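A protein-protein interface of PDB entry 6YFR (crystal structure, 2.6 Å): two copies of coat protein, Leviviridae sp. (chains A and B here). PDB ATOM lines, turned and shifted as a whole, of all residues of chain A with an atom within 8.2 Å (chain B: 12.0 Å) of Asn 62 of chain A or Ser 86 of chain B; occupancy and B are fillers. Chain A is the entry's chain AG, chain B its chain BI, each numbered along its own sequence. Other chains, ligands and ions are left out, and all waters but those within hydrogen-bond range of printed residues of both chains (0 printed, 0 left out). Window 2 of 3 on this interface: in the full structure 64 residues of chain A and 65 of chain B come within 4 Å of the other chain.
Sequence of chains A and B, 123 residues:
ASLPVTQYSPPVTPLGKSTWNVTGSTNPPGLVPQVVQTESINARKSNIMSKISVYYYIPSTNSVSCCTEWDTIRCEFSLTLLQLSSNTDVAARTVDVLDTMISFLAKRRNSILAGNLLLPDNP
O of Pro 59 of chain A is in hydrogen-bond range of ND2 of Asn 87 of chain B, 3.1 Å away.
O of Ser 60 of chain A lies within hydrogen-bond range of OG of Ser 85 of chain B, at 3.5 Å.
The backbone carbonyl oxygen (O) of Ser 60 of chain A sits at hydrogen-bond distance from the backbone NH (N) of Ser 86 of chain B.
N of Asn 87 of chain B sits at hydrogen-bond distance from O of Ser 60 of chain A (3.4 Å).
The backbone carbonyl oxygen (O) of Thr 61 of chain A sits at hydrogen-bond distance from the side-chain amide nitrogen (ND2) of Asn 87 of chain B (3.5 Å).
The side-chain amide nitrogen of Asn 62 of chain A lies within hydrogen-bond range of the backbone carbonyl oxygen of Ser 86 of chain B (3.1 Å).
The side-chain amide oxygen (OD1) of Asn 87 of chain B sits close to the side-chain amide oxygen (OD1) of Asn 62 of chain A (3.0 Å).
OD1 of Asn 62 of chain A is in hydrogen-bond range of N of Thr 88 of chain B.
No position is printed for both chains.
Of the 14 pairs that touch across the chains among the printed residues, none has its exchanged pair printed and touching as well.
Of the 10 printed residues of chain A, 6 touch a printed residue of chain B.
Hydrophobic or aromatic side chains of chain A that line the printed part of chain B: Ile 58 and Pro 59.
Of the printed residues of chain B, Ile 58 of chain A touches Leu 82 (3.9 Å), Asn 87 (3.5 Å), Asp 89 (3.97 Å) and Val 90 (3.9 Å).
Ser 60 of chain A touches just these residues of chain B: Ser 85 (3.5 Å), Ser 86 (3.2 Å) and Asn 87 (3.4 Å).
Of the printed residues of chain B, Thr 61 of chain A touches Asn 87.
Asn 62 of chain A touches three residues of chain B.
Thr 68 of chain A touches none of the printed residues of chain B.
Of the printed residues of chain B, Asp 71 of chain A touches Leu 82 (3.8 Å) and Ser 85 (3.8 Å).
Ser 86 of chain B touches two residues of chain A.
Printed residues of chain A within 4 Å of Thr 88 of chain B: Asn 62 (2.8 Å).
Of the printed residues of chain A, Val 90 of chain B touches Ile 58 (3.9 Å).
The nearest residue of chain B that does not touch Asn 62 of chain A is Asp 89 of chain B (4.3 Å).
The nearest residue of chain A that does not touch Ser 86 of chain B is Thr 61 of chain A (4.6 Å).
Ile 58 of chain A touches Leu 82 of chain B.
Ile 58 of chain A touches Asn 87 of chain B (CG1 to ND2, 3.5 Å).
Ile 58 of chain A touches Asp 89 of chain B (CD1 to CB, 3.97 Å).
Ile 58 of chain A touches Val 90 of chain B.
Leu 82 of chain B touches Asp 71 of chain A.
OD2 of Asp 71 of chain A touches OG of Ser 85 of chain B (3.8 Å).
N of Ile 58 of chain A lies within hydrogen-bond range of O of Asp 71 of chain A, 2.9 Å away.
OG1 of Thr 61 of chain A sits at hydrogen-bond distance from O of Ser 63 of chain A (2.7 Å).
The side-chain hydroxyl (OG1) of Thr 61 of chain A sits at hydrogen-bond distance from the side-chain hydroxyl (OG1) of Thr 68 of chain A, at 3.0 Å.
The backbone NH (N) of Asn 87 of chain B sits at hydrogen-bond distance from the side-chain hydroxyl (OG) of Ser 85 of chain B (3.3 Å).
The backbone NH (N) of Asp 89 of chain B is in hydrogen-bond range of the side-chain amide oxygen (OD1) of Asn 87 of chain B (2.7 Å).
The backbone carbonyl oxygen of Val 90 of chain B lies within hydrogen-bond range of the side-chain hydroxyl of Thr 94 of chain B (2.9 Å).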
ATOM      1  N   ILE A  58      12.981  29.821   6.424  1.00  0.00           N
ATOM      2  CA  ILE A  58      14.130  29.629   7.304  1.00  0.00           C
ATOM      3  C   ILE A  58      15.268  30.528   6.829  1.00  0.00           C
ATOM      4  O   ILE A  58      15.517  30.632   5.618  1.00  0.00           O
ATOM      5  CB  ILE A  58      14.535  28.144   7.353  1.00  0.00           C
ATOM      6  CG1 ILE A  58      15.644  27.899   8.375  1.00  0.00           C
ATOM      7  CG2 ILE A  58      14.944  27.636   5.972  1.00  0.00           C
ATOM      8  CD1 ILE A  58      15.945  26.427   8.588  1.00  0.00           C
ATOM      9  N   PRO A  59      15.961  31.217   7.734  1.00  0.00           N
ATOM     10  CA  PRO A  59      17.063  32.085   7.307  1.00  0.00           C
ATOM     11  C   PRO A  59      18.247  31.279   6.805  1.00  0.00           C
ATOM     12  O   PRO A  59      18.520  30.170   7.273  1.00  0.00           O
ATOM     13  CB  PRO A  59      17.418  32.865   8.580  1.00  0.00           C
ATOM     14  CG  PRO A  59      16.919  32.010   9.702  1.00  0.00           C
ATOM     15  CD  PRO A  59      15.685  31.338   9.176  1.00  0.00           C
ATOM     16  N   SER A  60      18.957  31.857   5.834  1.00  0.00           N
ATOM     17  CA  SER A  60      20.073  31.162   5.202  1.00  0.00           C
ATOM     18  C   SER A  60      21.251  30.965   6.145  1.00  0.00           C
ATOM     19  O   SER A  60      22.113  30.124   5.870  1.00  0.00           O
ATOM     20  CB  SER A  60      20.535  31.925   3.960  1.00  0.00           C
ATOM     21  OG  SER A  60      21.037  33.203   4.308  1.00  0.00           O
ATOM     22  N   THR A  61      21.313  31.720   7.238  1.00  0.00           N
ATOM     23  CA  THR A  61      22.391  31.613   8.207  1.00  0.00           C
ATOM     24  C   THR A  61      21.819  31.369   9.598  1.00  0.00           C
ATOM     25  O   THR A  61      20.631  31.585   9.854  1.00  0.00           O
ATOM     26  CB  THR A  61      23.260  32.877   8.214  1.00  0.00           C
ATOM     27  OG1 THR A  61      22.437  34.021   8.471  1.00  0.00           O
ATOM     28  CG2 THR A  61      23.959  33.050   6.874  1.00  0.00           C
ATOM     29  N   ASN A  62      22.688  30.909  10.502  1.00  0.00           N
ATOM     30  CA  ASN A  62      22.247  30.608  11.859  1.00  0.00           C
ATOM     31  C   ASN A  62      21.944  31.872  12.650  1.00  0.00           C
ATOM     32  O   ASN A  62      21.058  31.864  13.513  1.00  0.00           O
ATOM     33  CB  ASN A  62      23.305  29.771  12.578  1.00  0.00           C
ATOM     34  CG  ASN A  62      23.368  28.348  12.063  1.00  0.00           C
ATOM     35  OD1 ASN A  62      22.356  27.648  12.013  1.00  0.00           O
ATOM     36  ND2 ASN A  62      24.560  27.913  11.670  1.00  0.00           N
ATOM     37  N   SER A  63      22.653  32.962  12.374  1.00  0.00           N
ATOM     38  CA  SER A  63      22.470  34.220  13.079  1.00  0.00           C
ATOM     39  C   SER A  63      22.097  35.321  12.094  1.00  0.00           C
ATOM     40  O   SER A  63      22.146  35.143  10.874  1.00  0.00           O
ATOM     41  CB  SER A  63      23.734  34.605  13.854  1.00  0.00           C
ATOM     42  OG  SER A  63      23.563  35.847  14.511  1.00  0.00           O
ATOM     43  N   VAL A  64      21.721  36.475  12.644  1.00  0.00           N
ATOM     44  CA  VAL A  64      21.326  37.602  11.809  1.00  0.00           C
ATOM     45  C   VAL A  64      22.568  38.243  11.205  1.00  0.00           C
ATOM     46  O   VAL A  64      23.554  38.512  11.903  1.00  0.00           O
ATOM     47  CB  VAL A  64      20.508  38.615  12.623  1.00  0.00           C
ATOM     48  CG1 VAL A  64      19.898  39.664  11.702  1.00  0.00           C
ATOM     49  CG2 VAL A  64      19.427  37.905  13.423  1.00  0.00           C
ATOM     50  N   SER A  65      22.530  38.476   9.897  1.00  0.00           N
ATOM     51  CA  SER A  65      23.629  39.127   9.201  1.00  0.00           C
ATOM     52  C   SER A  65      23.059  39.923   8.035  1.00  0.00           C
ATOM     53  O   SER A  65      21.866  39.852   7.731  1.00  0.00           O
ATOM     54  CB  SER A  65      24.672  38.111   8.722  1.00  0.00           C
ATOM     55  OG  SER A  65      24.132  37.236   7.745  1.00  0.00           O
ATOM     56  N   THR A  68      21.943  37.797   5.099  1.00  0.00           N
ATOM     57  CA  THR A  68      20.955  36.792   5.466  1.00  0.00           C
ATOM     58  C   THR A  68      19.787  36.814   4.489  1.00  0.00           C
ATOM     59  O   THR A  68      19.056  37.805   4.405  1.00  0.00           O
ATOM     60  CB  THR A  68      20.459  37.036   6.891  1.00  0.00           C
ATOM     61  OG1 THR A  68      21.538  36.845   7.817  1.00  0.00           O
ATOM     62  CG2 THR A  68      19.320  36.092   7.238  1.00  0.00           C
ATOM     63  N   ASP A  71      15.424  31.278   2.773  1.00  0.00           N
ATOM     64  CA  ASP A  71      15.089  30.107   1.989  1.00  0.00           C
ATOM     65  C   ASP A  71      13.729  29.574   2.429  1.00  0.00           C
ATOM     66  O   ASP A  71      13.239  29.873   3.524  1.00  0.00           O
ATOM     67  CB  ASP A  71      16.162  29.028   2.146  1.00  0.00           C
ATOM     68  CG  ASP A  71      17.560  29.550   1.863  1.00  0.00           C
ATOM     69  OD1 ASP A  71      17.742  30.263   0.854  1.00  0.00           O
ATOM     70  OD2 ASP A  71      18.477  29.245   2.657  1.00  0.00           O
ATOM     71  N   LYS B  45      21.419  24.059  -8.426  1.00  0.00           N
ATOM     72  CA  LYS B  45      21.902  23.123  -7.409  1.00  0.00           C
ATOM     73  C   LYS B  45      21.671  23.648  -5.996  1.00  0.00           C
ATOM     74  O   LYS B  45      22.450  23.361  -5.083  1.00  0.00           O
ATOM     75  CB  LYS B  45      23.382  22.786  -7.613  1.00  0.00           C
ATOM     76  CG  LYS B  45      23.706  22.168  -8.965  1.00  0.00           C
ATOM     77  CD  LYS B  45      25.114  21.601  -8.963  1.00  0.00           C
ATOM     78  CE  LYS B  45      26.109  22.630  -8.451  1.00  0.00           C
ATOM     79  NZ  LYS B  45      27.473  22.060  -8.280  1.00  0.00           N
ATOM     80  N   SER B  46      20.606  24.424  -5.809  1.00  0.00           N
ATOM     81  CA  SER B  46      20.251  24.900  -4.481  1.00  0.00           C
ATOM     82  C   SER B  46      19.348  23.924  -3.741  1.00  0.00           C
ATOM     83  O   SER B  46      19.487  23.766  -2.523  1.00  0.00           O
ATOM     84  CB  SER B  46      19.574  26.271  -4.571  1.00  0.00           C
ATOM     85  OG  SER B  46      18.456  26.241  -5.441  1.00  0.00           O
ATOM     86  N   ASN B  47      18.442  23.252  -4.450  1.00  0.00           N
ATOM     87  CA  ASN B  47      17.504  22.328  -3.835  1.00  0.00           C
ATOM     88  C   ASN B  47      17.644  20.946  -4.455  1.00  0.00           C
ATOM     89  O   ASN B  47      17.975  20.808  -5.635  1.00  0.00           O
ATOM     90  CB  ASN B  47      16.046  22.792  -4.001  1.00  0.00           C
ATOM     91  CG  ASN B  47      15.741  24.056  -3.227  1.00  0.00           C
ATOM     92  OD1 ASN B  47      16.448  24.411  -2.286  1.00  0.00           O
ATOM     93  ND2 ASN B  47      14.671  24.739  -3.616  1.00  0.00           N
ATOM     94  N   LEU B  81      14.778  19.808  -0.235  1.00  0.00           N
ATOM     95  CA  LEU B  81      15.937  19.639   0.632  1.00  0.00           C
ATOM     96  C   LEU B  81      16.964  20.699   0.249  1.00  0.00           C
ATOM     97  O   LEU B  81      17.579  20.615  -0.822  1.00  0.00           O
ATOM     98  CB  LEU B  81      16.523  18.237   0.483  1.00  0.00           C
ATOM     99  CG  LEU B  81      15.543  17.066   0.560  1.00  0.00           C
ATOM    100  CD1 LEU B  81      16.287  15.742   0.474  1.00  0.00           C
ATOM    101  CD2 LEU B  81      14.723  17.146   1.832  1.00  0.00           C
ATOM    102  N   LEU B  82      17.136  21.700   1.108  1.00  0.00           N
ATOM    103  CA  LEU B  82      18.098  22.761   0.843  1.00  0.00           C
ATOM    104  C   LEU B  82      19.513  22.203   0.883  1.00  0.00           C
ATOM    105  O   LEU B  82      19.882  21.484   1.816  1.00  0.00           O
ATOM    106  CB  LEU B  82      17.942  23.881   1.869  1.00  0.00           C
ATOM    107  CG  LEU B  82      16.548  24.499   1.988  1.00  0.00           C
ATOM    108  CD1 LEU B  82      16.478  25.432   3.191  1.00  0.00           C
ATOM    109  CD2 LEU B  82      16.195  25.237   0.715  1.00  0.00           C
ATOM    110  N   GLN B  83      20.312  22.540  -0.132  1.00  0.00           N
ATOM    111  CA  GLN B  83      21.648  21.979  -0.284  1.00  0.00           C
ATOM    112  C   GLN B  83      22.770  22.970  -0.008  1.00  0.00           C
ATOM    113  O   GLN B  83      23.921  22.545   0.143  1.00  0.00           O
ATOM    114  CB  GLN B  83      21.827  21.411  -1.701  1.00  0.00           C
ATOM    115  CG  GLN B  83      20.870  20.290  -2.040  1.00  0.00           C
ATOM    116  CD  GLN B  83      21.134  19.042  -1.230  1.00  0.00           C
ATOM    117  OE1 GLN B  83      20.275  18.586  -0.473  1.00  0.00           O
ATOM    118  NE2 GLN B  83      22.325  18.477  -1.386  1.00  0.00           N
ATOM    119  N   LEU B  84      22.478  24.268   0.064  1.00  0.00           N
ATOM    120  CA  LEU B  84      23.525  25.277   0.180  1.00  0.00           C
ATOM    121  C   LEU B  84      23.265  26.224   1.342  1.00  0.00           C
ATOM    122  O   LEU B  84      23.743  27.360   1.343  1.00  0.00           O
ATOM    123  CB  LEU B  84      23.664  26.062  -1.125  1.00  0.00           C
ATOM    124  CG  LEU B  84      23.939  25.219  -2.372  1.00  0.00           C
ATOM    125  CD1 LEU B  84      24.019  26.097  -3.608  1.00  0.00           C
ATOM    126  CD2 LEU B  84      25.218  24.416  -2.195  1.00  0.00           C
ATOM    127  N   SER B  85      22.513  25.779   2.342  1.00  0.00           N
ATOM    128  CA  SER B  85      22.202  26.607   3.496  1.00  0.00           C
ATOM    129  C   SER B  85      23.202  26.348   4.614  1.00  0.00           C
ATOM    130  O   SER B  85      23.543  25.197   4.902  1.00  0.00           O
ATOM    131  CB  SER B  85      20.782  26.342   3.997  1.00  0.00           C
ATOM    132  OG  SER B  85      20.482  27.162   5.112  1.00  0.00           O
ATOM    133  N   SER B  86      23.669  27.428   5.238  1.00  0.00           N
ATOM    134  CA  SER B  86      24.554  27.335   6.392  1.00  0.00           C
ATOM    135  C   SER B  86      23.799  27.175   7.703  1.00  0.00           C
ATOM    136  O   SER B  86      24.430  26.952   8.742  1.00  0.00           O
ATOM    137  CB  SER B  86      25.450  28.575   6.473  1.00  0.00           C
ATOM    138  OG  SER B  86      26.220  28.721   5.292  1.00  0.00           O
ATOM    139  N   ASN B  87      22.474  27.290   7.681  1.00  0.00           N
ATOM    140  CA  ASN B  87      21.674  27.134   8.889  1.00  0.00           C
ATOM    141  C   ASN B  87      21.600  25.659   9.264  1.00  0.00           C
ATOM    142  O   ASN B  87      21.163  24.826   8.463  1.00  0.00           O
ATOM    143  CB  ASN B  87      20.276  27.712   8.671  1.00  0.00           C
ATOM    144  CG  ASN B  87      19.476  27.830   9.958  1.00  0.00           C
ATOM    145  OD1 ASN B  87      19.659  27.053  10.896  1.00  0.00           O
ATOM    146  ND2 ASN B  87      18.575  28.807  10.004  1.00  0.00           N
ATOM    147  N   THR B  88      22.027  25.334  10.483  1.00  0.00           N
ATOM    148  CA  THR B  88      22.012  23.952  10.945  1.00  0.00           C
ATOM    149  C   THR B  88      20.619  23.462  11.318  1.00  0.00           C
ATOM    150  O   THR B  88      20.450  22.263  11.563  1.00  0.00           O
ATOM    151  CB  THR B  88      22.951  23.791  12.142  1.00  0.00           C
ATOM    152  OG1 THR B  88      22.472  24.579  13.238  1.00  0.00           O
ATOM    153  CG2 THR B  88      24.358  24.247  11.772  1.00  0.00           C
ATOM    154  N   ASP B  89      19.620  24.350  11.363  1.00  0.00           N
ATOM    155  CA  ASP B  89      18.252  23.933  11.646  1.00  0.00           C
ATOM    156  C   ASP B  89      17.583  23.250  10.462  1.00  0.00           C
ATOM    157  O   ASP B  89      16.476  22.729  10.626  1.00  0.00           O
ATOM    158  CB  ASP B  89      17.393  25.133  12.056  1.00  0.00           C
ATOM    159  CG  ASP B  89      17.889  25.806  13.315  1.00  0.00           C
ATOM    160  OD1 ASP B  89      18.630  25.161  14.077  1.00  0.00           O
ATOM    161  OD2 ASP B  89      17.531  26.981  13.547  1.00  0.00           O
ATOM    162  N   VAL B  90      18.219  23.245   9.287  1.00  0.00           N
ATOM    163  CA  VAL B  90      17.534  22.824   8.067  1.00  0.00           C
ATOM    164  C   VAL B  90      17.057  21.381   8.176  1.00  0.00           C
ATOM    165  O   VAL B  90      15.933  21.057   7.780  1.00  0.00           O
ATOM    166  CB  VAL B  90      18.446  23.034   6.844  1.00  0.00           C
ATOM    167  CG1 VAL B  90      17.862  22.351   5.617  1.00  0.00           C
ATOM    168  CG2 VAL B  90      18.623  24.521   6.576  1.00  0.00           C
ATOM    169  N   ALA B  91      17.888  20.495   8.728  1.00  0.00           N
ATOM    170  CA  ALA B  91      17.513  19.084   8.792  1.00  0.00           C
ATOM    171  C   ALA B  91      16.314  18.867   9.708  1.00  0.00           C
ATOM    172  O   ALA B  91      15.315  18.248   9.311  1.00  0.00           O
ATOM    173  CB  ALA B  91      18.704  18.247   9.256  1.00  0.00           C
ATOM    174  N   ALA B  92      16.399  19.368  10.944  1.00  0.00           N
ATOM    175  CA  ALA B  92      15.298  19.199  11.883  1.00  0.00           C
ATOM    176  C   ALA B  92      14.028  19.862  11.374  1.00  0.00           C
ATOM    177  O   ALA B  92      12.928  19.333  11.570  1.00  0.00           O
ATOM    178  CB  ALA B  92      15.678  19.762  13.252  1.00  0.00           C
ATOM    179  N   ARG B  93      14.154  21.014  10.712  1.00  0.00           N
ATOM    180  CA  ARG B  93      12.965  21.701  10.225  1.00  0.00           C
ATOM    181  C   ARG B  93      12.358  21.005   9.013  1.00  0.00           C
ATOM    182  O   ARG B  93      11.135  21.000   8.872  1.00  0.00           O
ATOM    183  CB  ARG B  93      13.292  23.161   9.905  1.00  0.00           C
ATOM    184  CG  ARG B  93      13.648  24.011  11.130  1.00  0.00           C
ATOM    185  CD  ARG B  93      12.551  24.011  12.197  1.00  0.00           C
ATOM    186  NE  ARG B  93      12.671  22.896  13.137  1.00  0.00           N
ATOM    187  CZ  ARG B  93      13.447  22.909  14.215  1.00  0.00           C
ATOM    188  NH1 ARG B  93      14.175  23.982  14.499  1.00  0.00           N
ATOM    189  NH2 ARG B  93      13.496  21.847  15.009  1.00  0.00           N
ATOM    190  N   THR B  94      13.175  20.405   8.141  1.00  0.00           N
ATOM    191  CA  THR B  94      12.620  19.584   7.069  1.00  0.00           C
ATOM    192  C   THR B  94      11.879  18.383   7.641  1.00  0.00           C
ATOM    193  O   THR B  94      10.805  18.010   7.147  1.00  0.00           O
ATOM    194  CB  THR B  94      13.727  19.126   6.115  1.00  0.00           C
ATOM    195  OG1 THR B  94      14.813  18.576   6.871  1.00  0.00           O
ATOM    196  CG2 THR B  94      14.238  20.288   5.273  1.00  0.00           C
